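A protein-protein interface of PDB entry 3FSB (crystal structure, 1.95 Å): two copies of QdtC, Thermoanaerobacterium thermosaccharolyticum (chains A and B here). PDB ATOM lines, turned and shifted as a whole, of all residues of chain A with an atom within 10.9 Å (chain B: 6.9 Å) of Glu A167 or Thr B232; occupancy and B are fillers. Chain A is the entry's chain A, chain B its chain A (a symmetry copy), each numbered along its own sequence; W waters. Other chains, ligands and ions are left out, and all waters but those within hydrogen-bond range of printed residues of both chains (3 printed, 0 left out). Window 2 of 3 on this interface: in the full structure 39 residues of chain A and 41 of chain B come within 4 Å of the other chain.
The backbone carbonyl oxygen (O) of Val B236 sits at hydrogen-bond distance from the side-chain hydroxyl (OG1) of Thr B242 (2.5 Å). The side-chain carboxylate (OD2) of Asp A160 lies within hydrogen-bond range of the backbone NH (N) of Thr A162 (3.3 Å). The backbone carbonyl oxygen of Thr A162 lies close to the side-chain hydroxyl of Ser A165 (3.5 Å). N of Leu A169 sits at hydrogen-bond distance from O of Asn A159. N of Asn B229 sits at hydrogen-bond distance from O of Glu B234 (2.4 Å). OD1 of Asn B229 sits at hydrogen-bond distance from N of Thr B232, 3.0 Å away.
Pro A161 touches Lys B230 (CB to CG, 3.6 Å). Lys B230 touches Thr A162. Thr A162 touches Val B236 (OG1 to CG2, 3.4 Å). Asn A166 touches Thr B242 (OD1 to O, 3.6 Å). Ile B231 touches Glu A167. Glu A167 touches Thr B232 (OE2 to CG2, 3.3 Å). Leu A169 touches Ile B231.
Of chain B, only Asn B229, Ile B231 and Thr B232 come within 4 Å of Glu A167. Thr B232 touches one residue of chain A. Asn B229 touches just one residue of chain A: Glu A167 (3.4 Å). Of chain A, only Glu A167 and Leu A169 come within 4 Å of Ile B231. Of the printed residues of chain B, Asn A166 touches Thr B242 (3.6 Å). Of the printed residues of chain A, Thr B242 touches Asn A166. The nearest residue of chain B that does not touch Glu A167 is Thr B242 (6.7 Å). The nearest residue of chain A that does not touch Thr B232 is Asn A166 (7.8 Å).
Of the 10 printed residues of chain B, 6 touch a printed residue of chain A. Printed residues of chain B that touch a printed residue of chain A: Asn B229, Lys B230, Ile B231, Thr B232, Val B236 and Thr B242. Along chain B the printed residues that touch a printed residue of chain A span positions 229 to 242. Among the printed residues, no Asp or Glu carboxylate lies within 4 Å of a Lys or Arg side-chain nitrogen of the other chain.
No position is printed for both chains. Of the 8 pairs that touch across the chains among the printed residues, none has its exchanged pair printed and touching as well.
The side-chain carboxylate (OE1) of Glu A167 is in hydrogen-bond range of the side-chain amide nitrogen (ND2) of Asn B229.
Water W1 bridges the backbone carbonyl oxygen (O) of Pro A164 (2.6 Å) and the side-chain hydroxyl (OG1) of Thr B242 (3.1 Å). Water W3 lies within hydrogen-bond range of OG of Ser A165 (2.6 Å), O of Glu A167 (2.9 Å) and ND2 of Asn B229 (3.3 Å). Water W2 lies within hydrogen-bond range of OG1 of Thr A162 (2.8 Å), N of Lys B230 (2.8 Å) and OD1 of Asn B229 (3.2 Å).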
ATOM      1  N   GLU A 141      11.402  22.467   5.632  1.00  0.00           N
ATOM      2  CA  GLU A 141      12.640  23.195   5.364  1.00  0.00           C
ATOM      3  C   GLU A 141      12.684  23.631   3.891  1.00  0.00           C
ATOM      4  O   GLU A 141      12.145  22.955   2.982  1.00  0.00           O
ATOM      5  CB  GLU A 141      13.826  22.262   5.619  1.00  0.00           C
ATOM      6  CG  GLU A 141      13.493  20.851   5.210  1.00  0.00           C
ATOM      7  CD  GLU A 141      14.554  19.848   5.523  1.00  0.00           C
ATOM      8  OE1 GLU A 141      14.106  18.756   5.940  1.00  0.00           O
ATOM      9  OE2 GLU A 141      15.759  20.134   5.341  1.00  0.00           O
ATOM     10  N   LYS A 142      13.372  24.750   3.662  1.00  0.00           N
ATOM     11  CA  LYS A 142      13.551  25.391   2.342  1.00  0.00           C
ATOM     12  C   LYS A 142      12.329  26.069   1.762  1.00  0.00           C
ATOM     13  O   LYS A 142      12.370  26.536   0.607  1.00  0.00           O
ATOM     14  CB  LYS A 142      14.203  24.434   1.319  1.00  0.00           C
ATOM     15  CG  LYS A 142      15.449  23.689   1.780  1.00  0.00           C
ATOM     16  CD  LYS A 142      16.059  22.781   0.690  1.00  0.00           C
ATOM     17  CE  LYS A 142      16.665  23.548  -0.461  1.00  0.00           C
ATOM     18  NZ  LYS A 142      17.748  22.733  -1.019  1.00  0.00           N
ATOM     19  N   THR A 158       5.793  20.706   1.142  1.00  0.00           N
ATOM     20  CA  THR A 158       6.802  19.649   1.143  1.00  0.00           C
ATOM     21  C   THR A 158       8.066  20.070   0.454  1.00  0.00           C
ATOM     22  O   THR A 158       8.149  21.191  -0.010  1.00  0.00           O
ATOM     23  CB  THR A 158       6.255  18.448   0.373  1.00  0.00           C
ATOM     24  OG1 THR A 158       5.810  18.917  -0.904  1.00  0.00           O
ATOM     25  CG2 THR A 158       5.064  17.900   1.102  1.00  0.00           C
ATOM     26  N   ASN A 159       9.044  19.164   0.397  1.00  0.00           N
ATOM     27  CA  ASN A 159      10.343  19.495  -0.205  1.00  0.00           C
ATOM     28  C   ASN A 159      11.186  18.387  -0.830  1.00  0.00           C
ATOM     29  O   ASN A 159      12.173  18.664  -1.532  1.00  0.00           O
ATOM     30  CB  ASN A 159      11.190  20.276   0.785  1.00  0.00           C
ATOM     31  CG  ASN A 159      11.455  19.498   2.075  1.00  0.00           C
ATOM     32  OD1 ASN A 159      11.648  18.271   2.108  1.00  0.00           O
ATOM     33  ND2 ASN A 159      11.456  20.229   3.167  1.00  0.00           N
ATOM     34  N   ASP A 160      10.796  17.137  -0.607  1.00  0.00           N
ATOM     35  CA  ASP A 160      11.533  15.986  -1.193  1.00  0.00           C
ATOM     36  C   ASP A 160      10.759  15.431  -2.392  1.00  0.00           C
ATOM     37  O   ASP A 160       9.764  14.767  -2.227  1.00  0.00           O
ATOM     38  CB  ASP A 160      11.640  14.847  -0.178  1.00  0.00           C
ATOM     39  CG  ASP A 160      12.648  13.775  -0.618  1.00  0.00           C
ATOM     40  OD1 ASP A 160      13.216  13.078   0.237  1.00  0.00           O
ATOM     41  OD2 ASP A 160      12.829  13.617  -1.833  1.00  0.00           O
ATOM     42  N   PRO A 161      11.182  15.707  -3.610  1.00  0.00           N
ATOM     43  CA  PRO A 161      10.439  15.282  -4.775  1.00  0.00           C
ATOM     44  C   PRO A 161      10.312  13.821  -5.143  1.00  0.00           C
ATOM     45  O   PRO A 161       9.442  13.467  -5.937  1.00  0.00           O
ATOM     46  CB  PRO A 161      11.110  16.050  -5.916  1.00  0.00           C
ATOM     47  CG  PRO A 161      12.335  16.696  -5.296  1.00  0.00           C
ATOM     48  CD  PRO A 161      12.561  16.012  -3.999  1.00  0.00           C
ATOM     49  N   THR A 162      11.169  12.975  -4.591  1.00  0.00           N
ATOM     50  CA  THR A 162      11.089  11.545  -4.874  1.00  0.00           C
ATOM     51  C   THR A 162      11.649  10.954  -3.577  1.00  0.00           C
ATOM     52  O   THR A 162      12.798  10.537  -3.516  1.00  0.00           O
ATOM     53  CB  THR A 162      11.881  11.202  -6.160  1.00  0.00           C
ATOM     54  OG1 THR A 162      13.267  11.524  -6.020  1.00  0.00           O
ATOM     55  CG2 THR A 162      11.400  11.974  -7.355  1.00  0.00           C
ATOM     56  N   PRO A 163      10.858  11.035  -2.515  1.00  0.00           N
ATOM     57  CA  PRO A 163      11.254  10.596  -1.175  1.00  0.00           C
ATOM     58  C   PRO A 163      11.540   9.122  -0.956  1.00  0.00           C
ATOM     59  O   PRO A 163      10.831   8.300  -1.496  1.00  0.00           O
ATOM     60  CB  PRO A 163      10.081  11.064  -0.287  1.00  0.00           C
ATOM     61  CG  PRO A 163       8.892  11.240  -1.272  1.00  0.00           C
ATOM     62  CD  PRO A 163       9.398  11.024  -2.691  1.00  0.00           C
ATOM     63  N   PRO A 164      12.545   8.771  -0.155  1.00  0.00           N
ATOM     64  CA  PRO A 164      13.420   9.732   0.501  1.00  0.00           C
ATOM     65  C   PRO A 164      14.604   9.974  -0.420  1.00  0.00           C
ATOM     66  O   PRO A 164      15.107   8.999  -1.010  1.00  0.00           O
ATOM     67  CB  PRO A 164      13.926   8.918   1.688  1.00  0.00           C
ATOM     68  CG  PRO A 164      14.028   7.512   1.118  1.00  0.00           C
ATOM     69  CD  PRO A 164      12.684   7.432   0.432  1.00  0.00           C
ATOM     70  N   SER A 165      15.038  11.237  -0.535  1.00  0.00           N
ATOM     71  CA  SER A 165      16.187  11.564  -1.380  1.00  0.00           C
ATOM     72  C   SER A 165      17.082  12.625  -0.771  1.00  0.00           C
ATOM     73  O   SER A 165      16.717  13.284   0.196  1.00  0.00           O
ATOM     74  CB  SER A 165      15.839  11.883  -2.837  1.00  0.00           C
ATOM     75  OG  SER A 165      15.106  13.080  -2.959  1.00  0.00           O
ATOM     76  N   ASN A 166      18.244  12.812  -1.381  1.00  0.00           N
ATOM     77  CA  ASN A 166      19.205  13.759  -0.861  1.00  0.00           C
ATOM     78  C   ASN A 166      19.142  15.225  -1.272  1.00  0.00           C
ATOM     79  O   ASN A 166      19.740  16.059  -0.620  1.00  0.00           O
ATOM     80  CB  ASN A 166      20.629  13.197  -1.071  1.00  0.00           C
ATOM     81  CG  ASN A 166      20.828  11.885  -0.326  1.00  0.00           C
ATOM     82  OD1 ASN A 166      21.034  10.838  -0.940  1.00  0.00           O
ATOM     83  ND2 ASN A 166      20.714  11.937   0.992  1.00  0.00           N
ATOM     84  N   GLU A 167      18.429  15.525  -2.356  1.00  0.00           N
ATOM     85  CA  GLU A 167      18.357  16.886  -2.840  1.00  0.00           C
ATOM     86  C   GLU A 167      16.946  17.433  -2.678  1.00  0.00           C
ATOM     87  O   GLU A 167      16.066  17.102  -3.461  1.00  0.00           O
ATOM     88  CB  GLU A 167      18.818  16.887  -4.315  1.00  0.00           C
ATOM     89  CG  GLU A 167      20.236  16.258  -4.528  1.00  0.00           C
ATOM     90  CD  GLU A 167      20.240  14.750  -4.792  1.00  0.00           C
ATOM     91  OE1 GLU A 167      19.327  14.028  -4.330  1.00  0.00           O
ATOM     92  OE2 GLU A 167      21.153  14.284  -5.511  1.00  0.00           O
ATOM     93  N   LEU A 168      16.734  18.275  -1.666  1.00  0.00           N
ATOM     94  CA  LEU A 168      15.389  18.802  -1.492  1.00  0.00           C
ATOM     95  C   LEU A 168      15.139  20.088  -2.280  1.00  0.00           C
ATOM     96  O   LEU A 168      16.054  20.814  -2.603  1.00  0.00           O
ATOM     97  CB  LEU A 168      15.031  18.980  -0.020  1.00  0.00           C
ATOM     98  CG  LEU A 168      15.480  17.851   0.913  1.00  0.00           C
ATOM     99  CD1 LEU A 168      15.526  18.454   2.319  1.00  0.00           C
ATOM    100  CD2 LEU A 168      14.577  16.627   0.882  1.00  0.00           C
ATOM    101  N   LEU A 169      13.878  20.385  -2.581  1.00  0.00           N
ATOM    102  CA  LEU A 169      13.493  21.579  -3.331  1.00  0.00           C
ATOM    103  C   LEU A 169      12.339  22.238  -2.565  1.00  0.00           C
ATOM    104  O   LEU A 169      11.267  21.644  -2.380  1.00  0.00           O
ATOM    105  CB  LEU A 169      13.020  21.170  -4.730  1.00  0.00           C
ATOM    106  CG  LEU A 169      14.026  20.490  -5.665  1.00  0.00           C
ATOM    107  CD1 LEU A 169      13.290  19.983  -6.888  1.00  0.00           C
ATOM    108  CD2 LEU A 169      15.033  21.549  -6.106  1.00  0.00           C
ATOM    109  N   GLY A 170      12.595  23.457  -2.097  1.00  0.00           N
ATOM    110  CA  GLY A 170      11.630  24.234  -1.331  1.00  0.00           C
ATOM    111  C   GLY A 170      10.539  24.815  -2.206  1.00  0.00           C
ATOM    112  O   GLY A 170      10.736  25.133  -3.390  1.00  0.00           O
ATOM    113  N   VAL A 171       9.361  24.919  -1.605  1.00  0.00           N
ATOM    114  CA  VAL A 171       8.253  25.540  -2.334  1.00  0.00           C
ATOM    115  C   VAL A 171       8.381  27.070  -2.151  1.00  0.00           C
ATOM    116  O   VAL A 171       8.882  27.520  -1.112  1.00  0.00           O
ATOM    117  CB  VAL A 171       6.951  25.015  -1.703  1.00  0.00           C
ATOM    118  CG1 VAL A 171       5.732  25.855  -2.082  1.00  0.00           C
ATOM    119  CG2 VAL A 171       6.748  23.585  -2.135  1.00  0.00           C
ATOM    120  N   LEU A 186       3.458  20.173  -3.634  1.00  0.00           N
ATOM    121  CA  LEU A 186       4.601  19.317  -3.901  1.00  0.00           C
ATOM    122  C   LEU A 186       5.903  20.096  -3.979  1.00  0.00           C
ATOM    123  O   LEU A 186       5.924  21.317  -4.138  1.00  0.00           O
ATOM    124  CB  LEU A 186       4.378  18.503  -5.188  1.00  0.00           C
ATOM    125  CG  LEU A 186       3.565  17.217  -5.008  1.00  0.00           C
ATOM    126  CD1 LEU A 186       2.109  17.435  -4.509  1.00  0.00           C
ATOM    127  CD2 LEU A 186       3.501  16.443  -6.305  1.00  0.00           C
ATOM    128  N   PRO A 187       7.014  19.384  -3.864  1.00  0.00           N
ATOM    129  CA  PRO A 187       8.321  20.022  -3.900  1.00  0.00           C
ATOM    130  C   PRO A 187       8.720  20.868  -5.084  1.00  0.00           C
ATOM    131  O   PRO A 187       8.472  20.524  -6.241  1.00  0.00           O
ATOM    132  CB  PRO A 187       9.311  18.868  -3.686  1.00  0.00           C
ATOM    133  CG  PRO A 187       8.506  17.797  -3.017  1.00  0.00           C
ATOM    134  CD  PRO A 187       7.104  17.949  -3.524  1.00  0.00           C
ATOM    135  N   GLY A 188       9.365  21.982  -4.731  1.00  0.00           N
ATOM    136  CA  GLY A 188       9.925  22.948  -5.630  1.00  0.00           C
ATOM    137  C   GLY A 188       8.883  23.746  -6.363  1.00  0.00           C
ATOM    138  O   GLY A 188       9.228  24.565  -7.191  1.00  0.00           O
ATOM    139  N   LYS B 228      12.726   8.988 -11.898  1.00  0.00           N
ATOM    140  CA  LYS B 228      14.071   9.562 -12.068  1.00  0.00           C
ATOM    141  C   LYS B 228      14.269  10.719 -11.102  1.00  0.00           C
ATOM    142  O   LYS B 228      13.362  11.530 -10.880  1.00  0.00           O
ATOM    143  CB  LYS B 228      14.226  10.044 -13.505  1.00  0.00           C
ATOM    144  CG  LYS B 228      13.993   8.916 -14.516  1.00  0.00           C
ATOM    145  CD  LYS B 228      14.917   7.710 -14.269  1.00  0.00           C
ATOM    146  CE  LYS B 228      15.292   6.990 -15.566  1.00  0.00           C
ATOM    147  NZ  LYS B 228      14.313   5.961 -16.025  1.00  0.00           N
ATOM    148  N   ASN B 229      15.451  10.815 -10.515  1.00  0.00           N
ATOM    149  CA  ASN B 229      15.662  11.903  -9.589  1.00  0.00           C
ATOM    150  C   ASN B 229      15.456  13.212 -10.346  1.00  0.00           C
ATOM    151  O   ASN B 229      16.008  13.408 -11.421  1.00  0.00           O
ATOM    152  CB  ASN B 229      17.053  11.803  -9.000  1.00  0.00           C
ATOM    153  CG  ASN B 229      17.312  12.869  -7.960  1.00  0.00           C
ATOM    154  OD1 ASN B 229      17.362  14.048  -8.250  1.00  0.00           O
ATOM    155  ND2 ASN B 229      17.454  12.450  -6.737  1.00  0.00           N
ATOM    156  N   LYS B 230      14.644  14.103  -9.788  1.00  0.00           N
ATOM    157  CA  LYS B 230      14.338  15.385 -10.416  1.00  0.00           C
ATOM    158  C   LYS B 230      15.515  16.353 -10.608  1.00  0.00           C
ATOM    159  O   LYS B 230      15.460  17.291 -11.405  1.00  0.00           O
ATOM    160  CB  LYS B 230      13.180  16.059  -9.676  1.00  0.00           C
ATOM    161  CG  LYS B 230      12.112  15.068  -9.277  1.00  0.00           C
ATOM    162  CD  LYS B 230      10.720  15.518  -9.689  1.00  0.00           C
ATOM    163  CE  LYS B 230      10.649  15.687 -11.184  1.00  0.00           C
ATOM    164  NZ  LYS B 230      10.230  17.068 -11.552  1.00  0.00           N
ATOM    165  N   ILE B 231      16.591  16.115  -9.871  1.00  0.00           N
ATOM    166  CA  ILE B 231      17.753  16.972  -9.969  1.00  0.00           C
ATOM    167  C   ILE B 231      18.875  16.282 -10.731  1.00  0.00           C
ATOM    168  O   ILE B 231      19.546  16.910 -11.537  1.00  0.00           O
ATOM    169  CB  ILE B 231      18.204  17.392  -8.549  1.00  0.00           C
ATOM    170  CG1 ILE B 231      17.305  18.500  -8.011  1.00  0.00           C
ATOM    171  CG2 ILE B 231      19.750  17.557  -8.394  1.00  0.00           C
ATOM    172  CD1 ILE B 231      16.346  17.955  -6.962  1.00  0.00           C
ATOM    173  N   THR B 232      19.075  14.996 -10.476  1.00  0.00           N
ATOM    174  CA  THR B 232      20.139  14.268 -11.146  1.00  0.00           C
ATOM    175  C   THR B 232      19.712  13.365 -12.310  1.00  0.00           C
ATOM    176  O   THR B 232      20.585  12.943 -13.054  1.00  0.00           O
ATOM    177  CB  THR B 232      20.862  13.392 -10.165  1.00  0.00           C
ATOM    178  OG1 THR B 232      20.061  12.215  -9.978  1.00  0.00           O
ATOM    179  CG2 THR B 232      21.089  14.144  -8.843  1.00  0.00           C
ATOM    180  N   GLY B 233      18.418  13.047 -12.446  1.00  0.00           N
ATOM    181  CA  GLY B 233      17.915  12.233 -13.545  1.00  0.00           C
ATOM    182  C   GLY B 233      18.189  10.748 -13.406  1.00  0.00           C
ATOM    183  O   GLY B 233      17.914   9.962 -14.314  1.00  0.00           O
ATOM    184  N   GLU B 234      18.727  10.368 -12.255  1.00  0.00           N
ATOM    185  CA  GLU B 234      19.015   8.976 -12.010  1.00  0.00           C
ATOM    186  C   GLU B 234      17.778   8.290 -11.452  1.00  0.00           C
ATOM    187  O   GLU B 234      16.943   8.960 -10.873  1.00  0.00           O
ATOM    188  CB  GLU B 234      20.135   8.912 -10.987  1.00  0.00           C
ATOM    189  CG  GLU B 234      20.609   7.477 -10.723  1.00  0.00           C
ATOM    190  CD  GLU B 234      21.843   7.393  -9.829  1.00  0.00           C
ATOM    191  OE1 GLU B 234      22.575   8.410  -9.739  1.00  0.00           O
ATOM    192  OE2 GLU B 234      22.065   6.312  -9.216  1.00  0.00           O
ATOM    193  N   GLN B 235      17.674   6.971 -11.609  1.00  0.00           N
ATOM    194  CA  GLN B 235      16.552   6.170 -11.092  1.00  0.00           C
ATOM    195  C   GLN B 235      16.680   6.159  -9.567  1.00  0.00           C
ATOM    196  O   GLN B 235      17.728   5.855  -8.998  1.00  0.00           O
ATOM    197  CB  GLN B 235      16.579   4.722 -11.632  1.00  0.00           C
ATOM    198  CG  GLN B 235      15.722   3.744 -10.817  1.00  0.00           C
ATOM    199  CD  GLN B 235      15.697   2.345 -11.390  1.00  0.00           C
ATOM    200  OE1 GLN B 235      15.771   2.175 -12.612  1.00  0.00           O
ATOM    201  NE2 GLN B 235      15.542   1.337 -10.527  1.00  0.00           N
ATOM    202  N   VAL B 236      15.588   6.513  -8.908  1.00  0.00           N
ATOM    203  CA  VAL B 236      15.557   6.646  -7.463  1.00  0.00           C
ATOM    204  C   VAL B 236      15.301   5.394  -6.643  1.00  0.00           C
ATOM    205  O   VAL B 236      15.961   5.230  -5.605  1.00  0.00           O
ATOM    206  CB  VAL B 236      14.507   7.767  -7.079  1.00  0.00           C
ATOM    207  CG1 VAL B 236      14.345   8.010  -5.536  1.00  0.00           C
ATOM    208  CG2 VAL B 236      14.722   9.062  -7.882  1.00  0.00           C
ATOM    209  N   THR B 242      19.689   4.189  -3.326  1.00  0.00           N
ATOM    210  CA  THR B 242      20.046   5.568  -3.616  1.00  0.00           C
ATOM    211  C   THR B 242      20.048   6.481  -2.397  1.00  0.00           C
ATOM    212  O   THR B 242      20.450   7.653  -2.495  1.00  0.00           O
ATOM    213  CB  THR B 242      19.065   6.132  -4.626  1.00  0.00           C
ATOM    214  OG1 THR B 242      17.748   6.038  -4.065  1.00  0.00           O
ATOM    215  CG2 THR B 242      19.103   5.268  -5.868  1.00  0.00           C
HETATM  216  O   HOH W   1      16.863   8.801  -2.849  1.00  0.00           O
HETATM  217  O   HOH W   2      14.380  13.933  -6.969  1.00  0.00           O
HETATM  218  O   HOH W   3      15.722  14.627  -4.938  1.00  0.00           O
